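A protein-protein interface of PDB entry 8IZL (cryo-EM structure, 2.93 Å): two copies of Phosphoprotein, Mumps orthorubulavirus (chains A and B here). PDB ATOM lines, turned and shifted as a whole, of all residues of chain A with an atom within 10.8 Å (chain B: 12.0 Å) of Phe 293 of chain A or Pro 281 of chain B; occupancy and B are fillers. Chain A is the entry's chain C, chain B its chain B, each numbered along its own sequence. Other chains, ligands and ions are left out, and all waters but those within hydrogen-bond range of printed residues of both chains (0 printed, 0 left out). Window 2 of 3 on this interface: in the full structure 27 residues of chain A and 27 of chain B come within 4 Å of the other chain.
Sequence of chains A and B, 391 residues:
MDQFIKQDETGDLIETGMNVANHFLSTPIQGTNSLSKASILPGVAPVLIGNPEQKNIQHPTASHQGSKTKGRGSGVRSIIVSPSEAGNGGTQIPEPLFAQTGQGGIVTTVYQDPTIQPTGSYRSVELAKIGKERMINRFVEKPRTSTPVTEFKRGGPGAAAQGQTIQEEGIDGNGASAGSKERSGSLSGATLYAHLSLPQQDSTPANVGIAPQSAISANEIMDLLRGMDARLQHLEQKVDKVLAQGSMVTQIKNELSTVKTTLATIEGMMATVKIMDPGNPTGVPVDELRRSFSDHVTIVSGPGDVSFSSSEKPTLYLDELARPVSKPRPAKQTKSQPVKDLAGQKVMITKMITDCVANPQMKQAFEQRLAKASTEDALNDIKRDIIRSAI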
ATOM      1  N   LEU A 289       6.270  -1.670  26.474  1.00  0.00           N
ATOM      2  CA  LEU A 289       6.894  -2.049  25.210  1.00  0.00           C
ATOM      3  C   LEU A 289       7.731  -0.918  24.631  1.00  0.00           C
ATOM      4  O   LEU A 289       8.542  -1.145  23.738  1.00  0.00           O
ATOM      5  CB  LEU A 289       5.840  -2.464  24.187  1.00  0.00           C
ATOM      6  CG  LEU A 289       5.012  -3.708  24.484  1.00  0.00           C
ATOM      7  CD1 LEU A 289       4.053  -3.951  23.332  1.00  0.00           C
ATOM      8  CD2 LEU A 289       5.926  -4.907  24.675  1.00  0.00           C
ATOM      9  N   ARG A 290       7.534   0.298  25.121  1.00  0.00           N
ATOM     10  CA  ARG A 290       8.252   1.447  24.570  1.00  0.00           C
ATOM     11  C   ARG A 290       9.720   1.454  24.965  1.00  0.00           C
ATOM     12  O   ARG A 290      10.141   2.271  25.780  1.00  0.00           O
ATOM     13  CB  ARG A 290       7.581   2.756  24.988  1.00  0.00           C
ATOM     14  CG  ARG A 290       6.242   3.004  24.316  1.00  0.00           C
ATOM     15  CD  ARG A 290       5.470   4.111  25.010  1.00  0.00           C
ATOM     16  NE  ARG A 290       4.163   4.326  24.396  1.00  0.00           N
ATOM     17  CZ  ARG A 290       3.250   5.179  24.851  1.00  0.00           C
ATOM     18  NH1 ARG A 290       3.499   5.899  25.935  1.00  0.00           N
ATOM     19  NH2 ARG A 290       2.090   5.307  24.223  1.00  0.00           N
ATOM     20  N   ARG A 291      10.502   0.544  24.393  1.00  0.00           N
ATOM     21  CA  ARG A 291      11.932   0.516  24.656  1.00  0.00           C
ATOM     22  C   ARG A 291      12.602   0.733  23.324  1.00  0.00           C
ATOM     23  O   ARG A 291      13.260  -0.161  22.797  1.00  0.00           O
ATOM     24  CB  ARG A 291      12.356  -0.821  25.249  1.00  0.00           C
ATOM     25  CG  ARG A 291      13.807  -0.865  25.697  1.00  0.00           C
ATOM     26  CD  ARG A 291      14.209  -2.260  26.139  1.00  0.00           C
ATOM     27  NE  ARG A 291      15.588  -2.300  26.623  1.00  0.00           N
ATOM     28  CZ  ARG A 291      16.205  -3.402  27.029  1.00  0.00           C
ATOM     29  NH1 ARG A 291      15.569  -4.567  27.010  1.00  0.00           N
ATOM     30  NH2 ARG A 291      17.461  -3.344  27.456  1.00  0.00           N
ATOM     31  N   SER A 292      12.418   1.912  22.743  1.00  0.00           N
ATOM     32  CA  SER A 292      12.959   2.168  21.415  1.00  0.00           C
ATOM     33  C   SER A 292      13.278   3.637  21.206  1.00  0.00           C
ATOM     34  O   SER A 292      12.713   4.496  21.876  1.00  0.00           O
ATOM     35  CB  SER A 292      11.966   1.697  20.357  1.00  0.00           C
ATOM     36  OG  SER A 292      10.632   1.946  20.760  1.00  0.00           O
ATOM     37  N   PHE A 293      14.182   3.934  20.280  1.00  0.00           N
ATOM     38  CA  PHE A 293      14.592   5.314  20.074  1.00  0.00           C
ATOM     39  C   PHE A 293      13.461   6.176  19.578  1.00  0.00           C
ATOM     40  O   PHE A 293      12.713   5.765  18.699  1.00  0.00           O
ATOM     41  CB  PHE A 293      15.697   5.387  19.024  1.00  0.00           C
ATOM     42  CG  PHE A 293      17.016   4.835  19.473  1.00  0.00           C
ATOM     43  CD1 PHE A 293      17.089   3.829  20.419  1.00  0.00           C
ATOM     44  CD2 PHE A 293      18.191   5.322  18.931  1.00  0.00           C
ATOM     45  CE1 PHE A 293      18.307   3.323  20.823  1.00  0.00           C
ATOM     46  CE2 PHE A 293      19.414   4.823  19.330  1.00  0.00           C
ATOM     47  CZ  PHE A 293      19.473   3.823  20.279  1.00  0.00           C
ATOM     48  N   SER A 294      13.330   7.379  20.121  1.00  0.00           N
ATOM     49  CA  SER A 294      12.346   8.316  19.612  1.00  0.00           C
ATOM     50  C   SER A 294      13.019   9.221  18.607  1.00  0.00           C
ATOM     51  O   SER A 294      12.373  10.094  18.032  1.00  0.00           O
ATOM     52  CB  SER A 294      11.764   9.135  20.750  1.00  0.00           C
ATOM     53  OG  SER A 294      12.723  10.051  21.244  1.00  0.00           O
ATOM     54  N   ASP A 295      14.314   9.029  18.383  1.00  0.00           N
ATOM     55  CA  ASP A 295      15.063   9.946  17.525  1.00  0.00           C
ATOM     56  C   ASP A 295      15.659   9.340  16.274  1.00  0.00           C
ATOM     57  O   ASP A 295      16.291   8.287  16.328  1.00  0.00           O
ATOM     58  CB  ASP A 295      16.203  10.551  18.341  1.00  0.00           C
ATOM     59  CG  ASP A 295      16.748   9.587  19.371  1.00  0.00           C
ATOM     60  OD1 ASP A 295      16.358   9.697  20.551  1.00  0.00           O
ATOM     61  OD2 ASP A 295      17.555   8.711  18.998  1.00  0.00           O
ATOM     62  N   HIS A 296      15.456   9.999  15.139  1.00  0.00           N
ATOM     63  CA  HIS A 296      16.051   9.527  13.902  1.00  0.00           C
ATOM     64  C   HIS A 296      17.552   9.607  13.969  1.00  0.00           C
ATOM     65  O   HIS A 296      18.099  10.555  14.523  1.00  0.00           O
ATOM     66  CB  HIS A 296      15.585  10.376  12.729  1.00  0.00           C
ATOM     67  CG  HIS A 296      14.103  10.551  12.664  1.00  0.00           C
ATOM     68  ND1 HIS A 296      13.233   9.767  13.387  1.00  0.00           N
ATOM     69  CD2 HIS A 296      13.339  11.416  11.958  1.00  0.00           C
ATOM     70  CE1 HIS A 296      11.994  10.146  13.134  1.00  0.00           C
ATOM     71  NE2 HIS A 296      12.030  11.139  12.265  1.00  0.00           N
ATOM     72  N   VAL A 297      18.233   8.614  13.413  1.00  0.00           N
ATOM     73  CA  VAL A 297      19.684   8.670  13.352  1.00  0.00           C
ATOM     74  C   VAL A 297      20.086   8.658  11.893  1.00  0.00           C
ATOM     75  O   VAL A 297      19.673   7.774  11.156  1.00  0.00           O
ATOM     76  CB  VAL A 297      20.326   7.476  14.070  1.00  0.00           C
ATOM     77  CG1 VAL A 297      21.725   7.840  14.542  1.00  0.00           C
ATOM     78  CG2 VAL A 297      19.462   7.026  15.239  1.00  0.00           C
ATOM     79  N   THR A 298      20.919   9.601  11.475  1.00  0.00           N
ATOM     80  CA  THR A 298      21.263   9.693  10.060  1.00  0.00           C
ATOM     81  C   THR A 298      22.466   8.834   9.729  1.00  0.00           C
ATOM     82  O   THR A 298      23.551   9.350   9.468  1.00  0.00           O
ATOM     83  CB  THR A 298      21.531  11.147   9.631  1.00  0.00           C
ATOM     84  OG1 THR A 298      20.599  12.018  10.283  1.00  0.00           O
ATOM     85  CG2 THR A 298      21.379  11.292   8.127  1.00  0.00           C
ATOM     86  N   ILE A 299      22.281   7.524   9.746  1.00  0.00           N
ATOM     87  CA  ILE A 299      23.371   6.611   9.418  1.00  0.00           C
ATOM     88  C   ILE A 299      23.247   6.224   7.952  1.00  0.00           C
ATOM     89  O   ILE A 299      22.139   6.120   7.413  1.00  0.00           O
ATOM     90  CB  ILE A 299      23.379   5.370  10.333  1.00  0.00           C
ATOM     91  CG1 ILE A 299      22.386   4.312   9.855  1.00  0.00           C
ATOM     92  CG2 ILE A 299      23.080   5.763  11.764  1.00  0.00           C
ATOM     93  CD1 ILE A 299      22.805   2.903  10.195  1.00  0.00           C
ATOM     94  N   VAL A 300      24.389   6.053   7.299  1.00  0.00           N
ATOM     95  CA  VAL A 300      24.437   5.755   5.873  1.00  0.00           C
ATOM     96  C   VAL A 300      24.426   4.246   5.679  1.00  0.00           C
ATOM     97  O   VAL A 300      25.207   3.520   6.307  1.00  0.00           O
ATOM     98  CB  VAL A 300      25.678   6.396   5.223  1.00  0.00           C
ATOM     99  CG1 VAL A 300      26.919   6.136   6.066  1.00  0.00           C
ATOM    100  CG2 VAL A 300      25.866   5.878   3.811  1.00  0.00           C
ATOM    101  N   ALA B 271      24.647  -3.544   6.476  1.00  0.00           N
ATOM    102  CA  ALA B 271      24.095  -2.210   6.696  1.00  0.00           C
ATOM    103  C   ALA B 271      22.580  -2.221   6.576  1.00  0.00           C
ATOM    104  O   ALA B 271      21.878  -1.607   7.394  1.00  0.00           O
ATOM    105  CB  ALA B 271      24.706  -1.218   5.708  1.00  0.00           C
ATOM    106  N   THR B 272      22.065  -2.919   5.573  1.00  0.00           N
ATOM    107  CA  THR B 272      20.627  -2.996   5.380  1.00  0.00           C
ATOM    108  C   THR B 272      19.987  -3.664   6.576  1.00  0.00           C
ATOM    109  O   THR B 272      18.963  -3.215   7.074  1.00  0.00           O
ATOM    110  CB  THR B 272      20.265  -3.784   4.118  1.00  0.00           C
ATOM    111  OG1 THR B 272      20.936  -3.212   2.988  1.00  0.00           O
ATOM    112  CG2 THR B 272      18.767  -3.747   3.884  1.00  0.00           C
ATOM    113  N   VAL B 273      20.591  -4.744   7.047  1.00  0.00           N
ATOM    114  CA  VAL B 273      20.070  -5.420   8.218  1.00  0.00           C
ATOM    115  C   VAL B 273      20.020  -4.447   9.389  1.00  0.00           C
ATOM    116  O   VAL B 273      18.975  -4.286  10.013  1.00  0.00           O
ATOM    117  CB  VAL B 273      20.909  -6.653   8.588  1.00  0.00           C
ATOM    118  CG1 VAL B 273      20.534  -7.158   9.973  1.00  0.00           C
ATOM    119  CG2 VAL B 273      20.740  -7.742   7.541  1.00  0.00           C
ATOM    120  N   LYS B 274      21.136  -3.791   9.696  1.00  0.00           N
ATOM    121  CA  LYS B 274      21.128  -2.904  10.857  1.00  0.00           C
ATOM    122  C   LYS B 274      20.058  -1.827  10.731  1.00  0.00           C
ATOM    123  O   LYS B 274      19.349  -1.538  11.703  1.00  0.00           O
ATOM    124  CB  LYS B 274      22.500  -2.265  11.063  1.00  0.00           C
ATOM    125  CG  LYS B 274      22.495  -1.219  12.168  1.00  0.00           C
ATOM    126  CD  LYS B 274      23.878  -0.658  12.443  1.00  0.00           C
ATOM    127  CE  LYS B 274      23.782   0.693  13.128  1.00  0.00           C
ATOM    128  NZ  LYS B 274      23.941   0.575  14.603  1.00  0.00           N
ATOM    129  N   ILE B 275      19.883  -1.266   9.538  1.00  0.00           N
ATOM    130  CA  ILE B 275      18.880  -0.220   9.338  1.00  0.00           C
ATOM    131  C   ILE B 275      17.454  -0.763   9.279  1.00  0.00           C
ATOM    132  O   ILE B 275      16.515  -0.004   9.053  1.00  0.00           O
ATOM    133  CB  ILE B 275      19.146   0.607   8.060  1.00  0.00           C
ATOM    134  CG1 ILE B 275      19.003  -0.251   6.802  1.00  0.00           C
ATOM    135  CG2 ILE B 275      20.524   1.242   8.113  1.00  0.00           C
ATOM    136  CD1 ILE B 275      17.642  -0.177   6.144  1.00  0.00           C
ATOM    137  N   MET B 276      17.286  -2.065   9.475  1.00  0.00           N
ATOM    138  CA  MET B 276      15.953  -2.668   9.401  1.00  0.00           C
ATOM    139  C   MET B 276      15.340  -2.882  10.776  1.00  0.00           C
ATOM    140  O   MET B 276      14.281  -3.487  10.894  1.00  0.00           O
ATOM    141  CB  MET B 276      15.991  -4.000   8.651  1.00  0.00           C
ATOM    142  CG  MET B 276      15.893  -3.882   7.139  1.00  0.00           C
ATOM    143  SD  MET B 276      15.801  -5.500   6.348  1.00  0.00           S
ATOM    144  CE  MET B 276      15.525  -5.041   4.641  1.00  0.00           C
ATOM    145  N   ASP B 277      16.005  -2.389  11.815  1.00  0.00           N
ATOM    146  CA  ASP B 277      15.477  -2.517  13.168  1.00  0.00           C
ATOM    147  C   ASP B 277      14.560  -1.350  13.484  1.00  0.00           C
ATOM    148  O   ASP B 277      15.010  -0.210  13.570  1.00  0.00           O
ATOM    149  CB  ASP B 277      16.618  -2.580  14.181  1.00  0.00           C
ATOM    150  CG  ASP B 277      16.126  -2.710  15.609  1.00  0.00           C
ATOM    151  OD1 ASP B 277      14.943  -3.054  15.811  1.00  0.00           O
ATOM    152  OD2 ASP B 277      16.928  -2.471  16.536  1.00  0.00           O
ATOM    153  N   PRO B 278      13.263  -1.627  13.668  1.00  0.00           N
ATOM    154  CA  PRO B 278      12.294  -0.566  13.948  1.00  0.00           C
ATOM    155  C   PRO B 278      12.595   0.135  15.263  1.00  0.00           C
ATOM    156  O   PRO B 278      12.110   1.239  15.490  1.00  0.00           O
ATOM    157  CB  PRO B 278      10.969  -1.322  14.044  1.00  0.00           C
ATOM    158  CG  PRO B 278      11.189  -2.593  13.300  1.00  0.00           C
ATOM    159  CD  PRO B 278      12.622  -2.945  13.550  1.00  0.00           C
ATOM    160  N   GLY B 279      13.398  -0.492  16.111  1.00  0.00           N
ATOM    161  CA  GLY B 279      13.738   0.101  17.392  1.00  0.00           C
ATOM    162  C   GLY B 279      14.435   1.439  17.271  1.00  0.00           C
ATOM    163  O   GLY B 279      14.138   2.363  18.024  1.00  0.00           O
ATOM    164  N   ASN B 280      15.368   1.551  16.332  1.00  0.00           N
ATOM    165  CA  ASN B 280      16.105   2.795  16.151  1.00  0.00           C
ATOM    166  C   ASN B 280      15.796   3.426  14.805  1.00  0.00           C
ATOM    167  O   ASN B 280      16.268   2.950  13.777  1.00  0.00           O
ATOM    168  CB  ASN B 280      17.608   2.541  16.250  1.00  0.00           C
ATOM    169  CG  ASN B 280      18.006   1.869  17.548  1.00  0.00           C
ATOM    170  OD1 ASN B 280      17.165   1.341  18.276  1.00  0.00           O
ATOM    171  ND2 ASN B 280      19.298   1.878  17.842  1.00  0.00           N
ATOM    172  N   PRO B 281      15.007   4.508  14.805  1.00  0.00           N
ATOM    173  CA  PRO B 281      14.706   5.203  13.553  1.00  0.00           C
ATOM    174  C   PRO B 281      15.973   5.663  12.843  1.00  0.00           C
ATOM    175  O   PRO B 281      16.904   6.115  13.506  1.00  0.00           O
ATOM    176  CB  PRO B 281      13.870   6.395  14.014  1.00  0.00           C
ATOM    177  CG  PRO B 281      13.229   5.931  15.278  1.00  0.00           C
ATOM    178  CD  PRO B 281      14.254   5.059  15.943  1.00  0.00           C
ATOM    179  N   THR B 282      16.014   5.550  11.521  1.00  0.00           N
ATOM    180  CA  THR B 282      17.190   5.915  10.746  1.00  0.00           C
ATOM    181  C   THR B 282      16.850   7.027   9.765  1.00  0.00           C
ATOM    182  O   THR B 282      15.702   7.168   9.332  1.00  0.00           O
ATOM    183  CB  THR B 282      17.746   4.711   9.980  1.00  0.00           C
ATOM    184  OG1 THR B 282      16.660   3.890   9.528  1.00  0.00           O
ATOM    185  CG2 THR B 282      18.653   3.887  10.878  1.00  0.00           C
ATOM    186  N   GLY B 283      17.861   7.817   9.420  1.00  0.00           N
ATOM    187  CA  GLY B 283      17.689   8.895   8.469  1.00  0.00           C
ATOM    188  C   GLY B 283      18.655   8.821   7.304  1.00  0.00           C
ATOM    189  O   GLY B 283      19.850   8.587   7.495  1.00  0.00           O
ATOM    190  N   VAL B 284      18.146   9.009   6.097  1.00  0.00           N
ATOM    191  CA  VAL B 284      19.005   8.996   4.907  1.00  0.00           C
ATOM    192  C   VAL B 284      19.862  10.257   4.899  1.00  0.00           C
ATOM    193  O   VAL B 284      19.336  11.358   5.139  1.00  0.00           O
ATOM    194  CB  VAL B 284      18.155   8.904   3.641  1.00  0.00           C
ATOM    195  CG1 VAL B 284      18.988   8.400   2.484  1.00  0.00           C
ATOM    196  CG2 VAL B 284      16.967   7.998   3.874  1.00  0.00           C
ATOM    197  N   PRO B 285      21.167  10.157   4.656  1.00  0.00           N
ATOM    198  CA  PRO B 285      21.987  11.372   4.558  1.00  0.00           C
ATOM    199  C   PRO B 285      21.494  12.275   3.439  1.00  0.00           C
ATOM    200  O   PRO B 285      21.149  11.811   2.349  1.00  0.00           O
ATOM    201  CB  PRO B 285      23.392  10.828   4.270  1.00  0.00           C
ATOM    202  CG  PRO B 285      23.368   9.430   4.787  1.00  0.00           C
ATOM    203  CD  PRO B 285      21.977   8.933   4.548  1.00  0.00           C
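Among the printed residues, merely in contact across the chains: Ser 292 of chain A with Gly 279 of chain B (3.3 Å), Phe 293 of chain A with Asn 280 of chain B (3.1 Å), Phe 293 of chain A with Pro 281 of chain B (3.2 Å), Asp 295 of chain A with Pro 281 of chain B (3.6 Å), His 296 of chain A with Pro 281 of chain B (3.5 Å), Val 297 of chain A with Thr 282 of chain B (3.1 Å), Thr 298 of chain A with Gly 283 of chain B (3.1 Å), Thr 298 of chain A with Val 284 of chain B (3.6 Å), Thr 298 of chain A with Pro 285 of chain B (3.6 Å), Ile 299 of chain A with Lys 274 of chain B (3.8 Å), Ile 299 of chain A with Ile 275 of chain B (3.5 Å), Ile 299 of chain A with Thr 282 of chain B (3.9 Å) and Val 300 of chain A with Pro 285 of chain B (3.8 Å).
Of chain B, only Gly 279 (2.7 Å), Asn 280 (3.1 Å) and Pro 281 (3.2 Å) come within 4 Å of Phe 293 of chain A.
Pro 281 of chain B touches just these residues of chain A: Phe 293 (3.2 Å), Asp 295 (3.6 Å), His 296 (3.5 Å) and Val 297 (2.8 Å).
Ser 292 of chain A touches just one residue of chain B: Gly 279.
His 296 of chain A touches one residue of chain B.
Of chain A, only Phe 293 (3.1 Å) comes within 4 Å of Asn 280 of chain B.
Thr 282 of chain B touches just these residues of chain A: Val 297 and Ile 299.
Of the printed residues of chain A, Gly 283 of chain B touches Val 297, Thr 298 and Ile 299.
Printed residues of chain A within 4 Å of Val 284 of chain B: Thr 298.
Of the printed residues of chain B, Thr 298 of chain A touches Gly 283, Val 284 and Pro 285.
Leu 289 of chain A touches none of the printed residues of chain B.
The nearest residue of chain B that does not touch Phe 293 of chain A is Pro 278 of chain B (5.6 Å).
The nearest residue of chain A that does not touch Pro 281 of chain B is Ser 294 of chain A (4.7 Å).
The backbone carbonyl oxygen of Gly 279 of chain B lies within hydrogen-bond range of the backbone NH of Phe 293 of chain A, at 2.7 Å.
The backbone carbonyl oxygen of Pro 281 of chain B is in hydrogen-bond range of the backbone NH of Val 297 of chain A, at 2.8 Å.
The backbone carbonyl oxygen (O) of Val 297 of chain A sits at hydrogen-bond distance from the backbone NH (N) of Gly 283 of chain B.
The backbone carbonyl oxygen of Gly 283 of chain B sits at hydrogen-bond distance from the backbone NH of Ile 299 of chain A, at 3.5 Å.
No position is printed for both chains.
The side-chain carboxylate (OD1) of Asp 277 of chain B lies close to the backbone NH (N) of Gly 279 of chain B, 3.0 Å away.
Of the 12 printed residues of chain A, 8 touch a printed residue of chain B.
Printed residues of chain A that touch a printed residue of chain B: Ser 292, Phe 293, Asp 295, His 296, Val 297, Thr 298, Ile 299 and Val 300.
Hydrophobic or aromatic side chains of chain A within 4 Å of the printed part of chain B: Phe 293, His 296, Val 297, Ile 299 and Val 300.
Printed residues of chain B that touch a printed residue of chain A: Lys 274, Ile 275, Gly 279, Asn 280, Pro 281, Thr 282, Gly 283, Val 284 and Pro 285.
Among the printed residues, 17 pairs touch across the chains.
Among the printed residues, no Asp or Glu carboxylate lies within 4 Å of a Lys or Arg side-chain nitrogen of the other chain.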
